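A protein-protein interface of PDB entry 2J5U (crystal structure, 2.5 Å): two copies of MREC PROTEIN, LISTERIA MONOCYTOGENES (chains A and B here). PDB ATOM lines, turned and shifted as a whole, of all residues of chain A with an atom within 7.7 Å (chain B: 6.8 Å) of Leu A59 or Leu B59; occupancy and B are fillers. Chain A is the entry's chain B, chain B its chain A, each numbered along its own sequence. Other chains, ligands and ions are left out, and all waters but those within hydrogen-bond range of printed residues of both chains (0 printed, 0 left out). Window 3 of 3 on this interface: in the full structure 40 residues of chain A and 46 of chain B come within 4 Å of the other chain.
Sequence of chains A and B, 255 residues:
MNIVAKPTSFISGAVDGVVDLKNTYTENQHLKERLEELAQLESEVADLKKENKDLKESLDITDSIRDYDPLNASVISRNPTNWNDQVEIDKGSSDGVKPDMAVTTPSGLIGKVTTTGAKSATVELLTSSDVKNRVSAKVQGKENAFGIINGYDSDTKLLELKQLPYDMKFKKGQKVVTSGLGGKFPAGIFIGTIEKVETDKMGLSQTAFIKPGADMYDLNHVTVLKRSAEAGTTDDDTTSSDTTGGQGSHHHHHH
The side-chain amino group (NZ) of Lys B56 lies within salt-bridge range of the side-chain carboxylate (OE2) of Glu A51 (2.6 Å).
The side-chain hydroxyl (OG) of Ser B58 is in hydrogen-bond range of the backbone carbonyl oxygen (O) of Asp B54. N of Ile B61 sits at hydrogen-bond distance from O of Lys B56, 3.0 Å away. The side-chain carboxylate (OE2) of Glu A51 lies close to a ring nitrogen (NE2) of His A221, 3.5 Å away. The backbone carbonyl oxygen (O) of Ser A58 is in hydrogen-bond range of the side-chain hydroxyl (OG1) of Thr A62 (3.1 Å). O of Leu A59 is in hydrogen-bond range of OG1 of Thr A62 (2.6 Å). The side-chain amide nitrogen (ND2) of Asn A72 lies within hydrogen-bond range of the side-chain hydroxyl (OG1) of Thr A223 (3.0 Å).
Among the printed residues, merely in contact across the chains: Asn A72 with Leu B59, Leu A55 with Leu B59, Leu A55 with Ile B61, Asn A52 with Leu B55, Asn A72 with Asp B60, Leu A55 with Leu B55, Leu A59 with Ser B58, Leu A55 with Lys B56, His A221 with Ile B61, Leu A59 with Leu B59, Asn A72 with Ile B61 and Ser A58 with Leu B59.
Printed residues of chain B within 4 Å of Asn A52: Leu B55 (3.6 Å). Printed residues of chain B within 4 Å of Ser A58: Leu B59 (3.99 Å). Of the printed residues of chain B, Leu A59 touches Ser B58 (3.8 Å) and Leu B59 (3.9 Å). Thr A62 touches none of the printed residues of chain B. Printed residues of chain A within 4 Å of Leu B55: Asn A52 (3.6 Å) and Leu A55 (3.8 Å). Of the printed residues of chain A, Ser B58 touches Leu A59. Printed residues of chain A within 4 Å of Leu B59: Leu A55 (3.5 Å), Ser A58 (3.99 Å), Leu A59 (3.9 Å) and Asn A72 (3.2 Å). The nearest printed residue of chain A that does not touch Leu B59 is Thr A62 (4.2 Å). The nearest printed residue of chain A that does not touch Ile B61 is Ser A58 (6.5 Å).
Of the 9 printed residues of chain B, 6 touch a printed residue of chain A. Printed residues of chain B that touch a printed residue of chain A: Leu B55, Lys B56, Ser B58, Leu B59, Asp B60 and Ile B61. Hydrophobic or aromatic side chains of chain B that line the printed part of chain A: Leu B55, Leu B59 and Ile B61. Printed residues of chain A that touch a printed residue of chain B: Glu A51, Asn A52, Leu A55, Ser A58, Leu A59, Asn A72 and His A221. Among the printed residues, 13 pairs touch across the chains. Among the printed residues, Asp or Glu carboxylates within 4 Å of a Lys or Arg side-chain nitrogen of the other chain: Glu A51 with Lys B56.
Leu B55 touches its own counterpart, Leu A55. Leu A55 touches Leu B59, but with the chains exchanged Leu A59 does not touch Leu B55 (4.01 Å). Leu A55 touches Ile B61, but with the chains exchanged Ile A61 does not touch Leu B55 (10.7 Å). Ser A58 touches Leu B59, and with the chains exchanged Leu A59 touches Ser B58. Positions printed for both chains: 54, 55, 56, 57, 58, 59, 60, 61 and 62.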
ATOM      1  N   GLU A  51      -2.942   3.070 -17.632  1.00  0.00           N
ATOM      2  CA  GLU A  51      -3.672   1.901 -17.165  1.00  0.00           C
ATOM      3  C   GLU A  51      -2.796   0.990 -16.305  1.00  0.00           C
ATOM      4  O   GLU A  51      -3.280   0.326 -15.382  1.00  0.00           O
ATOM      5  CB  GLU A  51      -4.257   1.131 -18.354  1.00  0.00           C
ATOM      6  CG  GLU A  51      -5.235   0.045 -17.951  1.00  0.00           C
ATOM      7  CD  GLU A  51      -6.206  -0.291 -19.056  1.00  0.00           C
ATOM      8  OE1 GLU A  51      -6.849   0.645 -19.580  1.00  0.00           O
ATOM      9  OE2 GLU A  51      -6.334  -1.485 -19.394  1.00  0.00           O
ATOM     10  N   ASN A  52      -1.503   0.960 -16.602  1.00  0.00           N
ATOM     11  CA  ASN A  52      -0.606   0.130 -15.822  1.00  0.00           C
ATOM     12  C   ASN A  52      -0.405   0.737 -14.434  1.00  0.00           C
ATOM     13  O   ASN A  52      -0.487   0.038 -13.420  1.00  0.00           O
ATOM     14  CB  ASN A  52       0.731  -0.022 -16.542  1.00  0.00           C
ATOM     15  CG  ASN A  52       0.623  -0.883 -17.783  1.00  0.00           C
ATOM     16  OD1 ASN A  52      -0.041  -1.915 -17.776  1.00  0.00           O
ATOM     17  ND2 ASN A  52       1.288  -0.471 -18.849  1.00  0.00           N
ATOM     18  N   LYS A  53      -0.154   2.041 -14.389  1.00  0.00           N
ATOM     19  CA  LYS A  53       0.043   2.722 -13.121  1.00  0.00           C
ATOM     20  C   LYS A  53      -1.161   2.493 -12.217  1.00  0.00           C
ATOM     21  O   LYS A  53      -1.023   2.045 -11.076  1.00  0.00           O
ATOM     22  CB  LYS A  53       0.235   4.222 -13.350  1.00  0.00           C
ATOM     23  CG  LYS A  53       0.270   5.043 -12.081  1.00  0.00           C
ATOM     24  CD  LYS A  53       0.567   6.501 -12.381  1.00  0.00           C
ATOM     25  CE  LYS A  53       0.750   7.287 -11.083  1.00  0.00           C
ATOM     26  NZ  LYS A  53       1.209   8.695 -11.305  1.00  0.00           N
ATOM     27  N   ASP A  54      -2.345   2.791 -12.738  1.00  0.00           N
ATOM     28  CA  ASP A  54      -3.561   2.625 -11.962  1.00  0.00           C
ATOM     29  C   ASP A  54      -3.721   1.177 -11.514  1.00  0.00           C
ATOM     30  O   ASP A  54      -4.090   0.916 -10.370  1.00  0.00           O
ATOM     31  CB  ASP A  54      -4.796   3.065 -12.771  1.00  0.00           C
ATOM     32  CG  ASP A  54      -4.757   4.548 -13.180  1.00  0.00           C
ATOM     33  OD1 ASP A  54      -4.258   5.395 -12.399  1.00  0.00           O
ATOM     34  OD2 ASP A  54      -5.250   4.871 -14.284  1.00  0.00           O
ATOM     35  N   LEU A  55      -3.440   0.237 -12.414  1.00  0.00           N
ATOM     36  CA  LEU A  55      -3.569  -1.179 -12.093  1.00  0.00           C
ATOM     37  C   LEU A  55      -2.587  -1.629 -11.019  1.00  0.00           C
ATOM     38  O   LEU A  55      -2.921  -2.482 -10.193  1.00  0.00           O
ATOM     39  CB  LEU A  55      -3.411  -2.021 -13.357  1.00  0.00           C
ATOM     40  CG  LEU A  55      -4.666  -2.019 -14.239  1.00  0.00           C
ATOM     41  CD1 LEU A  55      -4.378  -2.697 -15.559  1.00  0.00           C
ATOM     42  CD2 LEU A  55      -5.799  -2.721 -13.519  1.00  0.00           C
ATOM     43  N   LYS A  56      -1.382  -1.060 -11.031  1.00  0.00           N
ATOM     44  CA  LYS A  56      -0.377  -1.393 -10.020  1.00  0.00           C
ATOM     45  C   LYS A  56      -0.945  -0.958  -8.676  1.00  0.00           C
ATOM     46  O   LYS A  56      -1.046  -1.759  -7.746  1.00  0.00           O
ATOM     47  CB  LYS A  56       0.932  -0.643 -10.266  1.00  0.00           C
ATOM     48  CG  LYS A  56       1.711  -1.071 -11.497  1.00  0.00           C
ATOM     49  CD  LYS A  56       2.761  -0.005 -11.846  1.00  0.00           C
ATOM     50  CE  LYS A  56       3.492  -0.300 -13.156  1.00  0.00           C
ATOM     51  NZ  LYS A  56       4.347  -1.521 -13.052  1.00  0.00           N
ATOM     52  N   GLU A  57      -1.312   0.319  -8.586  1.00  0.00           N
ATOM     53  CA  GLU A  57      -1.894   0.868  -7.365  1.00  0.00           C
ATOM     54  C   GLU A  57      -2.972  -0.052  -6.818  1.00  0.00           C
ATOM     55  O   GLU A  57      -3.121  -0.181  -5.610  1.00  0.00           O
ATOM     56  CB  GLU A  57      -2.497   2.247  -7.626  1.00  0.00           C
ATOM     57  CG  GLU A  57      -1.571   3.399  -7.339  1.00  0.00           C
ATOM     58  CD  GLU A  57      -2.167   4.733  -7.738  1.00  0.00           C
ATOM     59  OE1 GLU A  57      -3.337   4.991  -7.380  1.00  0.00           O
ATOM     60  OE2 GLU A  57      -1.464   5.528  -8.406  1.00  0.00           O
ATOM     61  N   SER A  58      -3.724  -0.691  -7.707  1.00  0.00           N
ATOM     62  CA  SER A  58      -4.774  -1.602  -7.284  1.00  0.00           C
ATOM     63  C   SER A  58      -4.206  -2.822  -6.576  1.00  0.00           C
ATOM     64  O   SER A  58      -4.748  -3.257  -5.568  1.00  0.00           O
ATOM     65  CB  SER A  58      -5.611  -2.065  -8.477  1.00  0.00           C
ATOM     66  OG  SER A  58      -6.662  -1.161  -8.759  1.00  0.00           O
ATOM     67  N   LEU A  59      -3.115  -3.372  -7.103  1.00  0.00           N
ATOM     68  CA  LEU A  59      -2.498  -4.549  -6.509  1.00  0.00           C
ATOM     69  C   LEU A  59      -2.007  -4.366  -5.081  1.00  0.00           C
ATOM     70  O   LEU A  59      -2.203  -5.242  -4.237  1.00  0.00           O
ATOM     71  CB  LEU A  59      -1.335  -5.030  -7.371  1.00  0.00           C
ATOM     72  CG  LEU A  59      -1.640  -6.203  -8.300  1.00  0.00           C
ATOM     73  CD1 LEU A  59      -0.354  -6.625  -8.987  1.00  0.00           C
ATOM     74  CD2 LEU A  59      -2.222  -7.372  -7.509  1.00  0.00           C
ATOM     75  N   ASP A  60      -1.371  -3.234  -4.808  1.00  0.00           N
ATOM     76  CA  ASP A  60      -0.835  -2.963  -3.477  1.00  0.00           C
ATOM     77  C   ASP A  60      -1.868  -2.985  -2.367  1.00  0.00           C
ATOM     78  O   ASP A  60      -1.646  -3.560  -1.301  1.00  0.00           O
ATOM     79  CB  ASP A  60      -0.141  -1.609  -3.455  1.00  0.00           C
ATOM     80  CG  ASP A  60       0.973  -1.527  -4.458  1.00  0.00           C
ATOM     81  OD1 ASP A  60       1.760  -0.561  -4.379  1.00  0.00           O
ATOM     82  OD2 ASP A  60       1.056  -2.429  -5.324  1.00  0.00           O
ATOM     83  N   ILE A  61      -2.999  -2.348  -2.618  1.00  0.00           N
ATOM     84  CA  ILE A  61      -4.046  -2.281  -1.627  1.00  0.00           C
ATOM     85  C   ILE A  61      -4.880  -3.560  -1.606  1.00  0.00           C
ATOM     86  O   ILE A  61      -5.854  -3.646  -0.868  1.00  0.00           O
ATOM     87  CB  ILE A  61      -4.949  -1.066  -1.911  1.00  0.00           C
ATOM     88  CG1 ILE A  61      -4.091   0.112  -2.396  1.00  0.00           C
ATOM     89  CG2 ILE A  61      -5.698  -0.660  -0.653  1.00  0.00           C
ATOM     90  CD1 ILE A  61      -3.016   0.586  -1.407  1.00  0.00           C
ATOM     91  N   THR A  62      -4.487  -4.562  -2.392  1.00  0.00           N
ATOM     92  CA  THR A  62      -5.242  -5.821  -2.472  1.00  0.00           C
ATOM     93  C   THR A  62      -5.427  -6.542  -1.136  1.00  0.00           C
ATOM     94  O   THR A  62      -6.553  -6.667  -0.642  1.00  0.00           O
ATOM     95  CB  THR A  62      -4.608  -6.816  -3.481  1.00  0.00           C
ATOM     96  OG1 THR A  62      -4.529  -6.208  -4.774  1.00  0.00           O
ATOM     97  CG2 THR A  62      -5.462  -8.076  -3.597  1.00  0.00           C
ATOM     98  N   ASP A  63      -4.333  -7.030  -0.560  1.00  0.00           N
ATOM     99  CA  ASP A  63      -4.402  -7.723   0.723  1.00  0.00           C
ATOM    100  C   ASP A  63      -4.949  -6.753   1.760  1.00  0.00           C
ATOM    101  O   ASP A  63      -5.600  -7.150   2.726  1.00  0.00           O
ATOM    102  CB  ASP A  63      -3.011  -8.205   1.127  1.00  0.00           C
ATOM    103  CG  ASP A  63      -2.383  -9.106   0.076  1.00  0.00           C
ATOM    104  OD1 ASP A  63      -2.956 -10.187  -0.200  1.00  0.00           O
ATOM    105  OD2 ASP A  63      -1.324  -8.731  -0.481  1.00  0.00           O
ATOM    106  N   SER A  64      -4.685  -5.472   1.530  1.00  0.00           N
ATOM    107  CA  SER A  64      -5.135  -4.397   2.399  1.00  0.00           C
ATOM    108  C   SER A  64      -6.655  -4.400   2.614  1.00  0.00           C
ATOM    109  O   SER A  64      -7.148  -3.816   3.576  1.00  0.00           O
ATOM    110  CB  SER A  64      -4.687  -3.056   1.806  1.00  0.00           C
ATOM    111  OG  SER A  64      -5.370  -1.965   2.395  1.00  0.00           O
ATOM    112  N   ASN A  72     -13.098  -6.822  -8.891  1.00  0.00           N
ATOM    113  CA  ASN A  72     -12.597  -5.814  -9.812  1.00  0.00           C
ATOM    114  C   ASN A  72     -13.461  -5.719 -11.047  1.00  0.00           C
ATOM    115  O   ASN A  72     -13.791  -6.734 -11.657  1.00  0.00           O
ATOM    116  CB  ASN A  72     -11.171  -6.146 -10.206  1.00  0.00           C
ATOM    117  CG  ASN A  72     -10.217  -5.958  -9.063  1.00  0.00           C
ATOM    118  OD1 ASN A  72      -9.158  -6.570  -9.018  1.00  0.00           O
ATOM    119  ND2 ASN A  72     -10.589  -5.094  -8.125  1.00  0.00           N
ATOM    120  N   PRO A 106      -8.368   2.915  -5.613  1.00  0.00           N
ATOM    121  CA  PRO A 106      -7.298   3.018  -4.622  1.00  0.00           C
ATOM    122  C   PRO A 106      -7.277   4.331  -3.853  1.00  0.00           C
ATOM    123  O   PRO A 106      -6.987   4.358  -2.662  1.00  0.00           O
ATOM    124  CB  PRO A 106      -6.044   2.802  -5.459  1.00  0.00           C
ATOM    125  CG  PRO A 106      -6.513   1.799  -6.452  1.00  0.00           C
ATOM    126  CD  PRO A 106      -7.851   2.374  -6.878  1.00  0.00           C
ATOM    127  N   HIS A 221     -10.998   1.555 -14.099  1.00  0.00           N
ATOM    128  CA  HIS A 221     -10.969   0.369 -13.265  1.00  0.00           C
ATOM    129  C   HIS A 221     -11.573   0.700 -11.910  1.00  0.00           C
ATOM    130  O   HIS A 221     -11.279   1.726 -11.309  1.00  0.00           O
ATOM    131  CB  HIS A 221      -9.537  -0.134 -13.157  1.00  0.00           C
ATOM    132  CG  HIS A 221      -9.017  -0.689 -14.448  1.00  0.00           C
ATOM    133  ND1 HIS A 221      -9.567  -1.802 -15.050  1.00  0.00           N
ATOM    134  CD2 HIS A 221      -8.035  -0.259 -15.278  1.00  0.00           C
ATOM    135  CE1 HIS A 221      -8.945  -2.035 -16.194  1.00  0.00           C
ATOM    136  NE2 HIS A 221      -8.012  -1.114 -16.356  1.00  0.00           N
ATOM    137  N   THR A 223     -13.468  -1.042  -8.027  1.00  0.00           N
ATOM    138  CA  THR A 223     -13.611  -2.204  -7.143  1.00  0.00           C
ATOM    139  C   THR A 223     -14.909  -2.276  -6.337  1.00  0.00           C
ATOM    140  O   THR A 223     -15.273  -1.334  -5.638  1.00  0.00           O
ATOM    141  CB  THR A 223     -12.460  -2.287  -6.147  1.00  0.00           C
ATOM    142  OG1 THR A 223     -11.228  -2.408  -6.860  1.00  0.00           O
ATOM    143  CG2 THR A 223     -12.626  -3.497  -5.253  1.00  0.00           C
ATOM    144  N   ASP B  54      -0.360  -8.929 -17.497  1.00  0.00           N
ATOM    145  CA  ASP B  54      -0.068  -9.591 -16.231  1.00  0.00           C
ATOM    146  C   ASP B  54      -0.870  -8.972 -15.107  1.00  0.00           C
ATOM    147  O   ASP B  54      -1.501  -9.681 -14.327  1.00  0.00           O
ATOM    148  CB  ASP B  54       1.417  -9.504 -15.893  1.00  0.00           C
ATOM    149  CG  ASP B  54       2.274 -10.262 -16.878  1.00  0.00           C
ATOM    150  OD1 ASP B  54       1.830 -11.340 -17.347  1.00  0.00           O
ATOM    151  OD2 ASP B  54       3.393  -9.785 -17.170  1.00  0.00           O
ATOM    152  N   LEU B  55      -0.835  -7.646 -15.026  1.00  0.00           N
ATOM    153  CA  LEU B  55      -1.569  -6.923 -14.000  1.00  0.00           C
ATOM    154  C   LEU B  55      -3.039  -7.324 -13.989  1.00  0.00           C
ATOM    155  O   LEU B  55      -3.589  -7.666 -12.938  1.00  0.00           O
ATOM    156  CB  LEU B  55      -1.459  -5.420 -14.236  1.00  0.00           C
ATOM    157  CG  LEU B  55      -0.092  -4.788 -14.008  1.00  0.00           C
ATOM    158  CD1 LEU B  55      -0.093  -3.353 -14.510  1.00  0.00           C
ATOM    159  CD2 LEU B  55       0.228  -4.847 -12.532  1.00  0.00           C
ATOM    160  N   LYS B  56      -3.674  -7.282 -15.160  1.00  0.00           N
ATOM    161  CA  LYS B  56      -5.086  -7.635 -15.268  1.00  0.00           C
ATOM    162  C   LYS B  56      -5.327  -9.077 -14.867  1.00  0.00           C
ATOM    163  O   LYS B  56      -6.441  -9.430 -14.475  1.00  0.00           O
ATOM    164  CB  LYS B  56      -5.610  -7.390 -16.688  1.00  0.00           C
ATOM    165  CG  LYS B  56      -5.911  -5.928 -16.997  1.00  0.00           C
ATOM    166  CD  LYS B  56      -6.196  -5.707 -18.475  1.00  0.00           C
ATOM    167  CE  LYS B  56      -6.465  -4.241 -18.763  1.00  0.00           C
ATOM    168  NZ  LYS B  56      -6.459  -3.925 -20.222  1.00  0.00           N
ATOM    169  N   GLU B  57      -4.288  -9.906 -14.968  1.00  0.00           N
ATOM    170  CA  GLU B  57      -4.398 -11.311 -14.581  1.00  0.00           C
ATOM    171  C   GLU B  57      -4.250 -11.432 -13.062  1.00  0.00           C
ATOM    172  O   GLU B  57      -4.897 -12.277 -12.437  1.00  0.00           O
ATOM    173  CB  GLU B  57      -3.334 -12.166 -15.292  1.00  0.00           C
ATOM    174  CG  GLU B  57      -3.558 -12.322 -16.805  1.00  0.00           C
ATOM    175  CD  GLU B  57      -2.642 -13.365 -17.453  1.00  0.00           C
ATOM    176  OE1 GLU B  57      -1.402 -13.261 -17.293  1.00  0.00           O
ATOM    177  OE2 GLU B  57      -3.166 -14.283 -18.131  1.00  0.00           O
ATOM    178  N   SER B  58      -3.404 -10.576 -12.479  1.00  0.00           N
ATOM    179  CA  SER B  58      -3.162 -10.552 -11.033  1.00  0.00           C
ATOM    180  C   SER B  58      -4.463 -10.164 -10.339  1.00  0.00           C
ATOM    181  O   SER B  58      -4.811 -10.699  -9.290  1.00  0.00           O
ATOM    182  CB  SER B  58      -2.073  -9.533 -10.697  1.00  0.00           C
ATOM    183  OG  SER B  58      -0.879  -9.814 -11.409  1.00  0.00           O
ATOM    184  N   LEU B  59      -5.163  -9.208 -10.939  1.00  0.00           N
ATOM    185  CA  LEU B  59      -6.458  -8.755 -10.453  1.00  0.00           C
ATOM    186  C   LEU B  59      -7.394  -9.632 -11.279  1.00  0.00           C
ATOM    187  O   LEU B  59      -6.953 -10.263 -12.241  1.00  0.00           O
ATOM    188  CB  LEU B  59      -6.640  -7.282 -10.801  1.00  0.00           C
ATOM    189  CG  LEU B  59      -5.494  -6.426 -10.257  1.00  0.00           C
ATOM    190  CD1 LEU B  59      -5.366  -5.121 -11.034  1.00  0.00           C
ATOM    191  CD2 LEU B  59      -5.731  -6.188  -8.780  1.00  0.00           C
ATOM    192  N   ASP B  60      -8.669  -9.707 -10.940  1.00  0.00           N
ATOM    193  CA  ASP B  60      -9.536 -10.565 -11.746  1.00  0.00           C
ATOM    194  C   ASP B  60     -10.203  -9.772 -12.863  1.00  0.00           C
ATOM    195  O   ASP B  60     -11.429  -9.623 -12.895  1.00  0.00           O
ATOM    196  CB  ASP B  60     -10.587 -11.229 -10.859  1.00  0.00           C
ATOM    197  CG  ASP B  60     -10.645 -12.722 -11.067  1.00  0.00           C
ATOM    198  OD1 ASP B  60      -9.566 -13.356 -11.034  1.00  0.00           O
ATOM    199  OD2 ASP B  60     -11.760 -13.258 -11.263  1.00  0.00           O
ATOM    200  N   ILE B  61      -9.388  -9.281 -13.790  1.00  0.00           N
ATOM    201  CA  ILE B  61      -9.897  -8.464 -14.879  1.00  0.00           C
ATOM    202  C   ILE B  61      -9.938  -9.115 -16.252  1.00  0.00           C
ATOM    203  O   ILE B  61      -8.910  -9.360 -16.887  1.00  0.00           O
ATOM    204  CB  ILE B  61      -9.103  -7.158 -14.969  1.00  0.00           C
ATOM    205  CG1 ILE B  61      -9.226  -6.406 -13.645  1.00  0.00           C
ATOM    206  CG2 ILE B  61      -9.617  -6.313 -16.116  1.00  0.00           C
ATOM    207  CD1 ILE B  61      -8.348  -5.189 -13.544  1.00  0.00           C
ATOM    208  N   THR B  62     -11.150  -9.374 -16.715  1.00  0.00           N
ATOM    209  CA  THR B  62     -11.355  -9.978 -18.016  1.00  0.00           C
ATOM    210  C   THR B  62     -12.117  -9.009 -18.906  1.00  0.00           C
ATOM    211  O   THR B  62     -12.864  -8.158 -18.418  1.00  0.00           O
ATOM    212  CB  THR B  62     -12.179 -11.261 -17.895  1.00  0.00           C
ATOM    213  OG1 THR B  62     -13.432 -10.959 -17.264  1.00  0.00           O
ATOM    214  CG2 THR B  62     -11.435 -12.288 -17.067  1.00  0.00           C
